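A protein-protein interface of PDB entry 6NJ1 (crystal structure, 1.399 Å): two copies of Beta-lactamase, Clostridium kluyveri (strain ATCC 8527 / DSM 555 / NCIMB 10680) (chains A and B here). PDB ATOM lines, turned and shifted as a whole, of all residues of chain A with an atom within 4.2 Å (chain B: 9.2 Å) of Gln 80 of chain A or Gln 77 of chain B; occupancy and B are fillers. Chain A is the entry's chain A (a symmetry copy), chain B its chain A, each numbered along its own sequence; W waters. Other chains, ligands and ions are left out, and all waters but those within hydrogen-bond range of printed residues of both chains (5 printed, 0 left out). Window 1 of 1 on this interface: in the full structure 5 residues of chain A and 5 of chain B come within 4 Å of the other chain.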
ATOM      1  N   ASP A  73       0.525 -33.478  31.855  1.00  0.00           N
ATOM      2  CA  ASP A  73       0.236 -32.675  30.678  1.00  0.00           C
ATOM      3  C   ASP A  73      -0.291 -33.503  29.504  1.00  0.00           C
ATOM      4  O   ASP A  73       0.072 -34.662  29.308  1.00  0.00           O
ATOM      5  CB  ASP A  73       1.529 -32.015  30.150  1.00  0.00           C
ATOM      6  CG  ASP A  73       1.975 -30.826  30.951  1.00  0.00           C
ATOM      7  OD1 ASP A  73       1.380 -30.509  32.022  1.00  0.00           O
ATOM      8  OD2 ASP A  73       2.946 -30.168  30.493  1.00  0.00           O
ATOM      9  N   GLU A  76      -0.439 -31.913  23.638  1.00  0.00           N
ATOM     10  CA  GLU A  76      -0.372 -30.558  23.106  1.00  0.00           C
ATOM     11  C   GLU A  76       0.233 -29.584  24.097  1.00  0.00           C
ATOM     12  O   GLU A  76       0.849 -28.585  23.690  1.00  0.00           O
ATOM     13  CB  GLU A  76      -1.750 -30.066  22.666  1.00  0.00           C
ATOM     14  CG  GLU A  76      -1.897 -30.094  21.126  1.00  0.00           C
ATOM     15  CD  GLU A  76      -0.889 -29.155  20.397  1.00  0.00           C
ATOM     16  OE1 GLU A  76      -0.586 -28.029  20.916  1.00  0.00           O
ATOM     17  OE2 GLU A  76      -0.382 -29.561  19.314  1.00  0.00           O
ATOM     18  N   GLN A  77       0.060 -29.834  25.392  1.00  0.00           N
ATOM     19  CA  GLN A  77       0.676 -28.972  26.401  1.00  0.00           C
ATOM     20  C   GLN A  77       2.193 -29.043  26.367  1.00  0.00           C
ATOM     21  O   GLN A  77       2.848 -28.133  26.877  1.00  0.00           O
ATOM     22  CB  GLN A  77       0.126 -29.272  27.810  1.00  0.00           C
ATOM     23  CG  GLN A  77      -1.245 -28.657  27.946  1.00  0.00           C
ATOM     24  CD  GLN A  77      -1.970 -28.994  29.208  1.00  0.00           C
ATOM     25  OE1 GLN A  77      -1.873 -30.143  29.726  1.00  0.00           O
ATOM     26  NE2 GLN A  77      -2.723 -28.005  29.722  1.00  0.00           N
ATOM     27  N   LEU A  78       2.760 -30.074  25.787  1.00  0.00           N
ATOM     28  CA  LEU A  78       4.223 -30.116  25.695  1.00  0.00           C
ATOM     29  C   LEU A  78       4.772 -29.045  24.745  1.00  0.00           C
ATOM     30  O   LEU A  78       5.978 -28.763  24.756  1.00  0.00           O
ATOM     31  CB  LEU A  78       4.674 -31.513  25.215  1.00  0.00           C
ATOM     32  CG  LEU A  78       4.348 -32.679  26.137  1.00  0.00           C
ATOM     33  CD1 LEU A  78       4.697 -34.003  25.437  1.00  0.00           C
ATOM     34  CD2 LEU A  78       5.048 -32.541  27.518  1.00  0.00           C
ATOM     35  N   LYS A  79       3.924 -28.466  23.906  1.00  0.00           N
ATOM     36  CA  LYS A  79       4.349 -27.438  22.971  1.00  0.00           C
ATOM     37  C   LYS A  79       4.264 -26.042  23.548  1.00  0.00           C
ATOM     38  O   LYS A  79       4.630 -25.081  22.873  1.00  0.00           O
ATOM     39  CB  LYS A  79       3.502 -27.455  21.696  1.00  0.00           C
ATOM     40  CG  LYS A  79       3.402 -28.796  21.054  1.00  0.00           C
ATOM     41  CD  LYS A  79       4.713 -29.236  20.508  1.00  0.00           C
ATOM     42  CE  LYS A  79       4.528 -30.255  19.392  1.00  0.00           C
ATOM     43  NZ  LYS A  79       5.662 -31.226  19.322  1.00  0.00           N
ATOM     44  N   GLN A  80       3.802 -25.903  24.784  1.00  0.00           N
ATOM     45  CA  GLN A  80       3.671 -24.573  25.369  1.00  0.00           C
ATOM     46  C   GLN A  80       5.043 -23.913  25.485  1.00  0.00           C
ATOM     47  O   GLN A  80       6.000 -24.521  25.986  1.00  0.00           O
ATOM     48  CB  GLN A  80       2.949 -24.585  26.728  1.00  0.00           C
ATOM     49  CG  GLN A  80       2.800 -23.151  27.245  1.00  0.00           C
ATOM     50  CD  GLN A  80       2.007 -23.028  28.501  1.00  0.00           C
ATOM     51  OE1 GLN A  80       1.700 -24.006  29.183  1.00  0.00           O
ATOM     52  NE2 GLN A  80       1.672 -21.791  28.836  1.00  0.00           N
ATOM     53  N   LEU A  81       5.133 -22.654  25.055  1.00  0.00           N
ATOM     54  CA  LEU A  81       6.370 -21.885  25.135  1.00  0.00           C
ATOM     55  C   LEU A  81       6.530 -21.229  26.506  1.00  0.00           C
ATOM     56  O   LEU A  81       5.589 -20.605  27.021  1.00  0.00           O
ATOM     57  CB  LEU A  81       6.334 -20.774  24.089  1.00  0.00           C
ATOM     58  CG  LEU A  81       7.662 -20.065  23.801  1.00  0.00           C
ATOM     59  CD1 LEU A  81       8.800 -20.977  23.348  1.00  0.00           C
ATOM     60  CD2 LEU A  81       7.463 -18.979  22.730  1.00  0.00           C
ATOM     61  N   VAL A  82       7.730 -21.343  27.071  1.00  0.00           N
ATOM     62  CA  VAL A  82       8.064 -20.782  28.385  1.00  0.00           C
ATOM     63  C   VAL A  82       9.135 -19.721  28.169  1.00  0.00           C
ATOM     64  O   VAL A  82      10.149 -19.991  27.503  1.00  0.00           O
ATOM     65  CB  VAL A  82       8.608 -21.867  29.345  1.00  0.00           C
ATOM     66  CG1 VAL A  82       9.076 -21.206  30.649  1.00  0.00           C
ATOM     67  CG2 VAL A  82       7.582 -22.914  29.587  1.00  0.00           C
ATOM     68  N   MET A 104      11.700 -21.412  25.456  1.00  0.00           N
ATOM     69  CA  MET A 104      11.808 -22.850  25.191  1.00  0.00           C
ATOM     70  C   MET A 104      10.453 -23.503  25.430  1.00  0.00           C
ATOM     71  O   MET A 104       9.736 -23.108  26.356  1.00  0.00           O
ATOM     72  CB  MET A 104      12.838 -23.526  26.118  1.00  0.00           C
ATOM     73  CG  MET A 104      14.241 -23.088  25.838  1.00  0.00           C
ATOM     74  SD  MET A 104      15.554 -23.880  27.028  1.00  0.00           S
ATOM     75  CE  MET A 104      15.350 -25.717  26.426  1.00  0.00           C
ATOM     76  N   THR A 105      10.103 -24.517  24.637  1.00  0.00           N
ATOM     77  CA  THR A 105       8.856 -25.221  24.922  1.00  0.00           C
ATOM     78  C   THR A 105       9.076 -26.250  26.029  1.00  0.00           C
ATOM     79  O   THR A 105      10.204 -26.625  26.367  1.00  0.00           O
ATOM     80  CB  THR A 105       8.357 -25.943  23.676  1.00  0.00           C
ATOM     81  OG1 THR A 105       9.315 -26.945  23.303  1.00  0.00           O
ATOM     82  CG2 THR A 105       8.136 -25.021  22.496  1.00  0.00           C
ATOM     83  N   ILE A 106       7.979 -26.744  26.579  1.00  0.00           N
ATOM     84  CA  ILE A 106       8.067 -27.746  27.639  1.00  0.00           C
ATOM     85  C   ILE A 106       8.844 -28.973  27.167  1.00  0.00           C
ATOM     86  O   ILE A 106       9.722 -29.487  27.889  1.00  0.00           O
ATOM     87  CB  ILE A 106       6.648 -28.100  28.142  1.00  0.00           C
ATOM     88  CG1 ILE A 106       5.965 -26.882  28.774  1.00  0.00           C
ATOM     89  CG2 ILE A 106       6.675 -29.294  29.095  1.00  0.00           C
ATOM     90  CD1 ILE A 106       6.650 -26.344  30.041  1.00  0.00           C
ATOM     91  N   HIS A 128       7.385 -26.176  36.333  1.00  0.00           N
ATOM     92  CA  HIS A 128       6.209 -26.608  35.598  1.00  0.00           C
ATOM     93  C   HIS A 128       5.382 -27.630  36.355  1.00  0.00           C
ATOM     94  O   HIS A 128       4.156 -27.711  36.128  1.00  0.00           O
ATOM     95  CB  HIS A 128       6.662 -27.181  34.265  1.00  0.00           C
ATOM     96  CG  HIS A 128       5.539 -27.474  33.346  1.00  0.00           C
ATOM     97  ND1 HIS A 128       4.802 -26.479  32.748  1.00  0.00           N
ATOM     98  CD2 HIS A 128       5.071 -28.648  32.848  1.00  0.00           C
ATOM     99  CE1 HIS A 128       3.899 -27.032  31.952  1.00  0.00           C
ATOM    100  NE2 HIS A 128       4.027 -28.344  32.020  1.00  0.00           N
ATOM    101  N   VAL B  69     -11.371 -27.088  32.793  1.00  0.00           N
ATOM    102  CA  VAL B  69     -10.098 -26.538  32.337  1.00  0.00           C
ATOM    103  C   VAL B  69      -9.287 -26.040  33.526  1.00  0.00           C
ATOM    104  O   VAL B  69      -8.100 -26.340  33.678  1.00  0.00           O
ATOM    105  CB  VAL B  69     -10.326 -25.388  31.325  1.00  0.00           C
ATOM    106  CG1 VAL B  69      -9.008 -24.651  31.075  1.00  0.00           C
ATOM    107  CG2 VAL B  69     -10.887 -25.905  30.026  1.00  0.00           C
ATOM    108  N   LEU B  70      -9.914 -25.271  34.388  1.00  0.00           N
ATOM    109  CA  LEU B  70      -9.213 -24.719  35.554  1.00  0.00           C
ATOM    110  C   LEU B  70      -8.705 -25.810  36.485  1.00  0.00           C
ATOM    111  O   LEU B  70      -7.610 -25.697  37.047  1.00  0.00           O
ATOM    112  CB  LEU B  70     -10.145 -23.755  36.288  1.00  0.00           C
ATOM    113  CG  LEU B  70     -10.425 -22.446  35.542  1.00  0.00           C
ATOM    114  CD1 LEU B  70     -11.597 -21.741  36.199  1.00  0.00           C
ATOM    115  CD2 LEU B  70      -9.240 -21.526  35.550  1.00  0.00           C
ATOM    116  N   LYS B  71      -9.458 -26.890  36.639  1.00  0.00           N
ATOM    117  CA  LYS B  71      -9.000 -27.947  37.525  1.00  0.00           C
ATOM    118  C   LYS B  71      -7.811 -28.703  36.923  1.00  0.00           C
ATOM    119  O   LYS B  71      -6.877 -29.094  37.633  1.00  0.00           O
ATOM    120  CB  LYS B  71     -10.160 -28.918  37.746  1.00  0.00           C
ATOM    121  CG  LYS B  71      -9.851 -30.128  38.624  1.00  0.00           C
ATOM    122  CD  LYS B  71      -9.459 -29.719  40.031  1.00  0.00           C
ATOM    123  CE  LYS B  71      -9.521 -30.858  41.007  1.00  0.00           C
ATOM    124  NZ  LYS B  71      -9.012 -30.462  42.362  1.00  0.00           N
ATOM    125  N   GLN B  72      -7.850 -28.900  35.606  1.00  0.00           N
ATOM    126  CA  GLN B  72      -6.832 -29.660  34.887  1.00  0.00           C
ATOM    127  C   GLN B  72      -5.509 -28.907  34.829  1.00  0.00           C
ATOM    128  O   GLN B  72      -4.440 -29.503  34.992  1.00  0.00           O
ATOM    129  CB  GLN B  72      -7.330 -29.861  33.460  1.00  0.00           C
ATOM    130  CG  GLN B  72      -6.359 -30.611  32.569  1.00  0.00           C
ATOM    131  CD  GLN B  72      -6.865 -30.784  31.146  1.00  0.00           C
ATOM    132  OE1 GLN B  72      -7.568 -31.754  30.849  1.00  0.00           O
ATOM    133  NE2 GLN B  72      -6.530 -29.838  30.265  1.00  0.00           N
ATOM    134  N   ASP B  73      -5.571 -27.594  34.602  1.00  0.00           N
ATOM    135  CA  ASP B  73      -4.448 -26.780  34.168  1.00  0.00           C
ATOM    136  C   ASP B  73      -3.888 -25.890  35.280  1.00  0.00           C
ATOM    137  O   ASP B  73      -4.606 -25.418  36.162  1.00  0.00           O
ATOM    138  CB  ASP B  73      -4.893 -25.799  33.061  1.00  0.00           C
ATOM    139  CG  ASP B  73      -5.055 -26.438  31.712  1.00  0.00           C
ATOM    140  OD1 ASP B  73      -4.944 -27.691  31.573  1.00  0.00           O
ATOM    141  OD2 ASP B  73      -5.287 -25.665  30.745  1.00  0.00           O
ATOM    142  N   SER B  74      -2.581 -25.647  35.234  1.00  0.00           N
ATOM    143  CA  SER B  74      -2.014 -24.600  36.073  1.00  0.00           C
ATOM    144  C   SER B  74      -2.411 -23.233  35.529  1.00  0.00           C
ATOM    145  O   SER B  74      -2.934 -23.102  34.408  1.00  0.00           O
ATOM    146  CB  SER B  74      -0.503 -24.692  36.050  1.00  0.00           C
ATOM    147  OG  SER B  74      -0.047 -24.328  34.750  1.00  0.00           O
ATOM    148  N   LEU B  75      -2.209 -22.215  36.355  1.00  0.00           N
ATOM    149  CA  LEU B  75      -2.476 -20.860  35.909  1.00  0.00           C
ATOM    150  C   LEU B  75      -1.635 -20.514  34.700  1.00  0.00           C
ATOM    151  O   LEU B  75      -2.131 -19.901  33.759  1.00  0.00           O
ATOM    152  CB  LEU B  75      -2.248 -19.858  37.048  1.00  0.00           C
ATOM    153  CG  LEU B  75      -3.279 -19.917  38.186  1.00  0.00           C
ATOM    154  CD1 LEU B  75      -2.900 -18.857  39.235  1.00  0.00           C
ATOM    155  CD2 LEU B  75      -4.694 -19.713  37.729  1.00  0.00           C
ATOM    156  N   GLU B  76      -0.378 -20.967  34.658  1.00  0.00           N
ATOM    157  CA  GLU B  76       0.433 -20.622  33.498  1.00  0.00           C
ATOM    158  C   GLU B  76      -0.035 -21.332  32.241  1.00  0.00           C
ATOM    159  O   GLU B  76       0.137 -20.805  31.129  1.00  0.00           O
ATOM    160  CB  GLU B  76       1.911 -20.920  33.744  1.00  0.00           C
ATOM    161  CG  GLU B  76       2.712 -19.626  34.022  1.00  0.00           C
ATOM    162  CD  GLU B  76       2.703 -18.630  32.823  1.00  0.00           C
ATOM    163  OE1 GLU B  76       2.750 -19.079  31.629  1.00  0.00           O
ATOM    164  OE2 GLU B  76       2.624 -17.396  33.082  1.00  0.00           O
ATOM    165  N   GLN B  77      -0.607 -22.524  32.384  1.00  0.00           N
ATOM    166  CA  GLN B  77      -1.143 -23.232  31.221  1.00  0.00           C
ATOM    167  C   GLN B  77      -2.320 -22.500  30.597  1.00  0.00           C
ATOM    168  O   GLN B  77      -2.636 -22.754  29.435  1.00  0.00           O
ATOM    169  CB  GLN B  77      -1.502 -24.691  31.565  1.00  0.00           C
ATOM    170  CG  GLN B  77      -0.235 -25.508  31.631  1.00  0.00           C
ATOM    171  CD  GLN B  77      -0.410 -26.914  32.104  1.00  0.00           C
ATOM    172  OE1 GLN B  77      -1.246 -27.195  33.011  1.00  0.00           O
ATOM    173  NE2 GLN B  77       0.383 -27.825  31.512  1.00  0.00           N
ATOM    174  N   LEU B  78      -2.959 -21.610  31.318  1.00  0.00           N
ATOM    175  CA  LEU B  78      -4.055 -20.855  30.700  1.00  0.00           C
ATOM    176  C   LEU B  78      -3.551 -19.890  29.620  1.00  0.00           C
ATOM    177  O   LEU B  78      -4.349 -19.381  28.821  1.00  0.00           O
ATOM    178  CB  LEU B  78      -4.819 -20.067  31.785  1.00  0.00           C
ATOM    179  CG  LEU B  78      -5.523 -20.895  32.850  1.00  0.00           C
ATOM    180  CD1 LEU B  78      -6.076 -19.966  33.944  1.00  0.00           C
ATOM    181  CD2 LEU B  78      -6.623 -21.809  32.241  1.00  0.00           C
ATOM    182  N   LYS B  79      -2.257 -19.604  29.598  1.00  0.00           N
ATOM    183  CA  LYS B  79      -1.686 -18.703  28.612  1.00  0.00           C
ATOM    184  C   LYS B  79      -1.246 -19.411  27.349  1.00  0.00           C
ATOM    185  O   LYS B  79      -0.778 -18.758  26.416  1.00  0.00           O
ATOM    186  CB  LYS B  79      -0.466 -17.963  29.168  1.00  0.00           C
ATOM    187  CG  LYS B  79      -0.710 -17.289  30.473  1.00  0.00           C
ATOM    188  CD  LYS B  79      -1.664 -16.158  30.330  1.00  0.00           C
ATOM    189  CE  LYS B  79      -1.481 -15.142  31.449  1.00  0.00           C
ATOM    190  NZ  LYS B  79      -2.758 -14.450  31.797  1.00  0.00           N
ATOM    191  N   GLN B  80      -1.392 -20.728  27.286  1.00  0.00           N
ATOM    192  CA  GLN B  80      -0.950 -21.456  26.102  1.00  0.00           C
ATOM    193  C   GLN B  80      -1.749 -21.007  24.881  1.00  0.00           C
ATOM    194  O   GLN B  80      -2.987 -20.942  24.921  1.00  0.00           O
ATOM    195  CB  GLN B  80      -1.022 -22.984  26.276  1.00  0.00           C
ATOM    196  CG  GLN B  80      -0.490 -23.672  25.017  1.00  0.00           C
ATOM    197  CD  GLN B  80      -0.399 -25.156  25.117  1.00  0.00           C
ATOM    198  OE1 GLN B  80      -0.922 -25.787  26.036  1.00  0.00           O
ATOM    199  NE2 GLN B  80       0.270 -25.747  24.138  1.00  0.00           N
ATOM    200  N   LEU B  81      -1.047 -20.731  23.783  1.00  0.00           N
ATOM    201  CA  LEU B  81      -1.676 -20.324  22.530  1.00  0.00           C
ATOM    202  C   LEU B  81      -2.124 -21.535  21.713  1.00  0.00           C
ATOM    203  O   LEU B  81      -1.355 -22.492  21.529  1.00  0.00           O
ATOM    204  CB  LEU B  81      -0.665 -19.545  21.694  1.00  0.00           C
ATOM    205  CG  LEU B  81      -1.224 -18.767  20.499  1.00  0.00           C
ATOM    206  CD1 LEU B  81      -2.304 -17.741  20.840  1.00  0.00           C
ATOM    207  CD2 LEU B  81      -0.087 -18.037  19.762  1.00  0.00           C
ATOM    208  N   VAL B  82      -3.350 -21.473  21.198  1.00  0.00           N
ATOM    209  CA  VAL B  82      -3.946 -22.542  20.392  1.00  0.00           C
ATOM    210  C   VAL B  82      -4.182 -21.985  18.995  1.00  0.00           C
ATOM    211  O   VAL B  82      -4.776 -20.903  18.852  1.00  0.00           O
ATOM    212  CB  VAL B  82      -5.296 -23.016  20.985  1.00  0.00           C
ATOM    213  CG1 VAL B  82      -5.945 -24.029  20.030  1.00  0.00           C
ATOM    214  CG2 VAL B  82      -5.101 -23.579  22.346  1.00  0.00           C
ATOM    215  N   MET B 104      -5.678 -18.225  19.647  1.00  0.00           N
ATOM    216  CA  MET B 104      -6.298 -17.777  20.899  1.00  0.00           C
ATOM    217  C   MET B 104      -5.670 -18.532  22.063  1.00  0.00           C
ATOM    218  O   MET B 104      -5.364 -19.721  21.928  1.00  0.00           O
ATOM    219  CB  MET B 104      -7.816 -18.047  20.913  1.00  0.00           C
ATOM    220  CG  MET B 104      -8.560 -17.208  19.922  1.00  0.00           C
ATOM    221  SD  MET B 104     -10.467 -17.567  19.878  1.00  0.00           S
ATOM    222  CE  MET B 104     -10.876 -16.918  21.664  1.00  0.00           C
ATOM    223  N   THR B 105      -5.505 -17.877  23.213  1.00  0.00           N
ATOM    224  CA  THR B 105      -5.004 -18.618  24.366  1.00  0.00           C
ATOM    225  C   THR B 105      -6.147 -19.375  25.039  1.00  0.00           C
ATOM    226  O   THR B 105      -7.334 -19.115  24.816  1.00  0.00           O
ATOM    227  CB  THR B 105      -4.385 -17.663  25.382  1.00  0.00           C
ATOM    228  OG1 THR B 105      -5.405 -16.782  25.874  1.00  0.00           O
ATOM    229  CG2 THR B 105      -3.258 -16.830  24.812  1.00  0.00           C
ATOM    230  N   ILE B 106      -5.785 -20.306  25.908  1.00  0.00           N
ATOM    231  CA  ILE B 106      -6.793 -21.085  26.623  1.00  0.00           C
ATOM    232  C   ILE B 106      -7.732 -20.173  27.409  1.00  0.00           C
ATOM    233  O   ILE B 106      -8.967 -20.349  27.374  1.00  0.00           O
ATOM    234  CB  ILE B 106      -6.100 -22.137  27.520  1.00  0.00           C
ATOM    235  CG1 ILE B 106      -5.309 -23.146  26.680  1.00  0.00           C
ATOM    236  CG2 ILE B 106      -7.100 -22.828  28.446  1.00  0.00           C
ATOM    237  CD1 ILE B 106      -6.163 -24.011  25.741  1.00  0.00           C
ATOM    238  N   GLU B 107      -7.196 -19.155  28.077  1.00  0.00           N
ATOM    239  CA  GLU B 107      -8.091 -18.291  28.845  1.00  0.00           C
ATOM    240  C   GLU B 107      -8.989 -17.488  27.909  1.00  0.00           C
ATOM    241  O   GLU B 107     -10.162 -17.249  28.221  1.00  0.00           O
ATOM    242  CB  GLU B 107      -7.285 -17.400  29.790  1.00  0.00           C
ATOM    243  CG  GLU B 107      -6.321 -16.479  29.226  1.00  0.00           C
ATOM    244  CD  GLU B 107      -5.543 -15.766  30.354  1.00  0.00           C
ATOM    245  OE1 GLU B 107      -5.953 -15.863  31.538  1.00  0.00           O
ATOM    246  OE2 GLU B 107      -4.519 -15.128  30.070  1.00  0.00           O
ATOM    247  N   GLU B 108      -8.464 -17.053  26.748  1.00  0.00           N
ATOM    248  CA  GLU B 108      -9.309 -16.353  25.775  1.00  0.00           C
ATOM    249  C   GLU B 108     -10.420 -17.246  25.248  1.00  0.00           C
ATOM    250  O   GLU B 108     -11.556 -16.796  25.003  1.00  0.00           O
ATOM    251  CB  GLU B 108      -8.470 -15.849  24.603  1.00  0.00           C
ATOM    252  CG  GLU B 108      -7.672 -14.632  24.968  1.00  0.00           C
ATOM    253  CD  GLU B 108      -6.548 -14.296  23.996  1.00  0.00           C
ATOM    254  OE1 GLU B 108      -6.229 -15.059  23.064  1.00  0.00           O
ATOM    255  OE2 GLU B 108      -5.920 -13.219  24.187  1.00  0.00           O
ATOM    256  N   ILE B 109     -10.113 -18.522  25.036  1.00  0.00           N
ATOM    257  CA  ILE B 109     -11.112 -19.498  24.614  1.00  0.00           C
ATOM    258  C   ILE B 109     -12.199 -19.654  25.666  1.00  0.00           C
ATOM    259  O   ILE B 109     -13.395 -19.662  25.338  1.00  0.00           O
ATOM    260  CB  ILE B 109     -10.387 -20.817  24.325  1.00  0.00           C
ATOM    261  CG1 ILE B 109      -9.636 -20.722  22.983  1.00  0.00           C
ATOM    262  CG2 ILE B 109     -11.352 -22.003  24.291  1.00  0.00           C
ATOM    263  CD1 ILE B 109      -8.554 -21.740  22.788  1.00  0.00           C
ATOM    264  N   CYS B 110     -11.819 -19.834  26.929  1.00  0.00           N
ATOM    265  CA  CYS B 110     -12.808 -19.968  27.982  1.00  0.00           C
ATOM    266  C   CYS B 110     -13.659 -18.723  28.099  1.00  0.00           C
ATOM    267  O   CYS B 110     -14.883 -18.815  28.240  1.00  0.00           O
ATOM    268  CB  CYS B 110     -12.112 -20.225  29.314  1.00  0.00           C
ATOM    269  SG  CYS B 110     -11.364 -21.874  29.448  1.00  0.00           S
ATOM    270  N   HIS B 128      -9.514 -29.244  24.494  1.00  0.00           N
ATOM    271  CA  HIS B 128      -8.478 -29.085  25.500  1.00  0.00           C
ATOM    272  C   HIS B 128      -8.658 -30.013  26.686  1.00  0.00           C
ATOM    273  O   HIS B 128      -7.655 -30.364  27.344  1.00  0.00           O
ATOM    274  CB  HIS B 128      -8.479 -27.636  25.960  1.00  0.00           C
ATOM    275  CG  HIS B 128      -7.336 -27.305  26.843  1.00  0.00           C
ATOM    276  ND1 HIS B 128      -6.046 -27.229  26.372  1.00  0.00           N
ATOM    277  CD2 HIS B 128      -7.288 -26.945  28.151  1.00  0.00           C
ATOM    278  CE1 HIS B 128      -5.247 -26.876  27.369  1.00  0.00           C
ATOM    279  NE2 HIS B 128      -5.975 -26.727  28.459  1.00  0.00           N
ATOM    280  N   LYS B 190      -8.593 -19.597  41.188  1.00  0.00           N
ATOM    281  CA  LYS B 190      -9.318 -20.187  40.063  1.00  0.00           C
ATOM    282  C   LYS B 190     -10.822 -19.994  40.189  1.00  0.00           C
ATOM    283  O   LYS B 190     -11.487 -19.744  39.185  1.00  0.00           O
ATOM    284  CB  LYS B 190      -8.955 -21.645  39.912  1.00  0.00           C
ATOM    285  CG  LYS B 190      -7.535 -21.840  39.427  1.00  0.00           C
ATOM    286  CD  LYS B 190      -7.193 -23.334  39.353  1.00  0.00           C
ATOM    287  CE  LYS B 190      -5.837 -23.576  38.802  1.00  0.00           C
ATOM    288  NZ  LYS B 190      -5.517 -25.034  38.730  1.00  0.00           N
HETATM  289  O   HOH W   1      -1.761 -25.481  21.145  1.00  0.00           O
HETATM  290  O   HOH W   2      -2.450 -25.432  28.311  1.00  0.00           O
HETATM  291  O   HOH W   3       2.517 -25.103  34.556  1.00  0.00           O
HETATM  292  O   HOH W   4       1.993 -26.751  29.291  1.00  0.00           O
HETATM  293  O   HOH W   5       4.708 -20.110  29.890  1.00  0.00           O
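Of the 23 printed residues of chain B, 5 touch a printed residue of chain A.
Hydrophobic or aromatic side chains of chain B that line the printed part of chain A: His 128.
Of the 12 printed residues of chain A, 5 touch a printed residue of chain B.
Hydrophobic or aromatic side chains of chain A within 4 Å of the printed part of chain B: His 128.
Along chain A the printed residues that touch a printed residue of chain B span positions 73 to 128.
Among the printed residues, no Asp or Glu carboxylate lies within 4 Å of a Lys or Arg side-chain nitrogen of the other chain.
Of the printed residues of chain B, Gln 77 of chain A touches Asp 73 (2.9 Å), Gln 77 (3.5 Å), Gln 80 (3.5 Å) and His 128 (3.6 Å).
Of chain B, only Glu 76, Gln 77 and Gln 80 come within 4 Å of Gln 80 of chain A.
Of the printed residues of chain B, His 128 of chain A touches Gln 77.
Of the printed residues of chain A, Asp 73 of chain B touches Gln 77 (2.9 Å).
Gln 77 of chain B touches four residues of chain A.
Of the printed residues of chain A, Gln 80 of chain B touches Glu 76, Gln 77 and Gln 80.
Glu 107 of chain B touches none of the printed residues of chain A.
The nearest printed residue of chain A that does not touch Gln 77 of chain B is Ile 106 of chain A (6.3 Å).
The nearest printed residue of chain B that does not touch Asp 73 of chain A is Gln 72 of chain B (6.6 Å).
Water W3 bridges OG of Ser 74 of chain B (2.7 Å) and ND1 of His 128 of chain A (3.2 Å).
Water W2 lies within hydrogen-bond range of OE1 of Gln 80 of chain B (2.8 Å), O of Gln 77 of chain B (2.9 Å) and NE2 of Gln 77 of chain A (2.9 Å).
Water W5 bridges the side-chain carboxylate (OE1) of Glu 76 of chain B (2.8 Å) and the backbone carbonyl oxygen (O) of Leu 81 of chain A (3.0 Å).
Water W1 bridges the side-chain carboxylate (OE1) of Glu 76 of chain A (2.8 Å) and the backbone carbonyl oxygen (O) of Leu 81 of chain B (3.0 Å).
The side-chain amide nitrogen of Gln 72 of chain B is in hydrogen-bond range of the side-chain carboxylate of Asp 73 of chain B, at 3.0 Å.
The side-chain amide nitrogen (NE2) of Gln 72 of chain B is in hydrogen-bond range of the backbone carbonyl oxygen (O) of His 128 of chain B (3.2 Å).
NE2 of His 128 of chain B sits at hydrogen-bond distance from OD2 of Asp 73 of chain B, at 2.6 Å.
O of Asp 73 of chain B sits at hydrogen-bond distance from NZ of Lys 190 of chain B, 2.8 Å away.
The side-chain hydroxyl (OG) of Ser 74 of chain B sits close to the backbone NH (N) of Glu 76 of chain B (3.4 Å).
NE2 of His 128 of chain A sits at hydrogen-bond distance from OD2 of Asp 73 of chain A (2.6 Å).
Among the printed residues, pairs that only touch across the chains: Gln 77 of chain A with Gln 77 of chain B (3.5 Å), Gln 77 of chain A with Gln 80 of chain B (3.5 Å), Gln 77 of chain A with His 128 of chain B (3.6 Å), Gln 80 of chain A with Gln 77 of chain B (3.5 Å), Gln 80 of chain A with Gln 80 of chain B (3.6 Å) and His 128 of chain A with Gln 77 of chain B (3.6 Å).
Asp 73 of chain A touches Gln 77 of chain B, and with the chains exchanged Gln 77 of chain A touches Asp 73 of chain B.
Glu 76 of chain A touches Gln 80 of chain B, and with the chains exchanged Gln 80 of chain A touches Glu 76 of chain B.
Gln 77 of chain B touches its own counterpart, Gln 77 of chain A.
Gln 77 of chain A touches Gln 80 of chain B, and with the chains exchanged Gln 80 of chain A touches Gln 77 of chain B.
Positions printed for both chains: 73, 76, 77, 78, 79, 80, 81, 82, 104, 105, 106 and 128.
Of the 10 pairs that touch across the chains among the printed residues, 10 have their exchanged pair printed and touching as well.
The side-chain amide nitrogen (NE2) of Gln 77 of chain A sits at hydrogen-bond distance from the side-chain carboxylate (OD1) of Asp 73 of chain B (2.9 Å).
NE2 of Gln 80 of chain A sits at hydrogen-bond distance from O of Glu 76 of chain B.
The side-chain carboxylate (OD1) of Asp 73 of chain A sits at hydrogen-bond distance from the side-chain amide nitrogen (NE2) of Gln 77 of chain B (2.9 Å).
NE2 of Gln 80 of chain B is in hydrogen-bond range of O of Glu 76 of chain A (2.9 Å).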
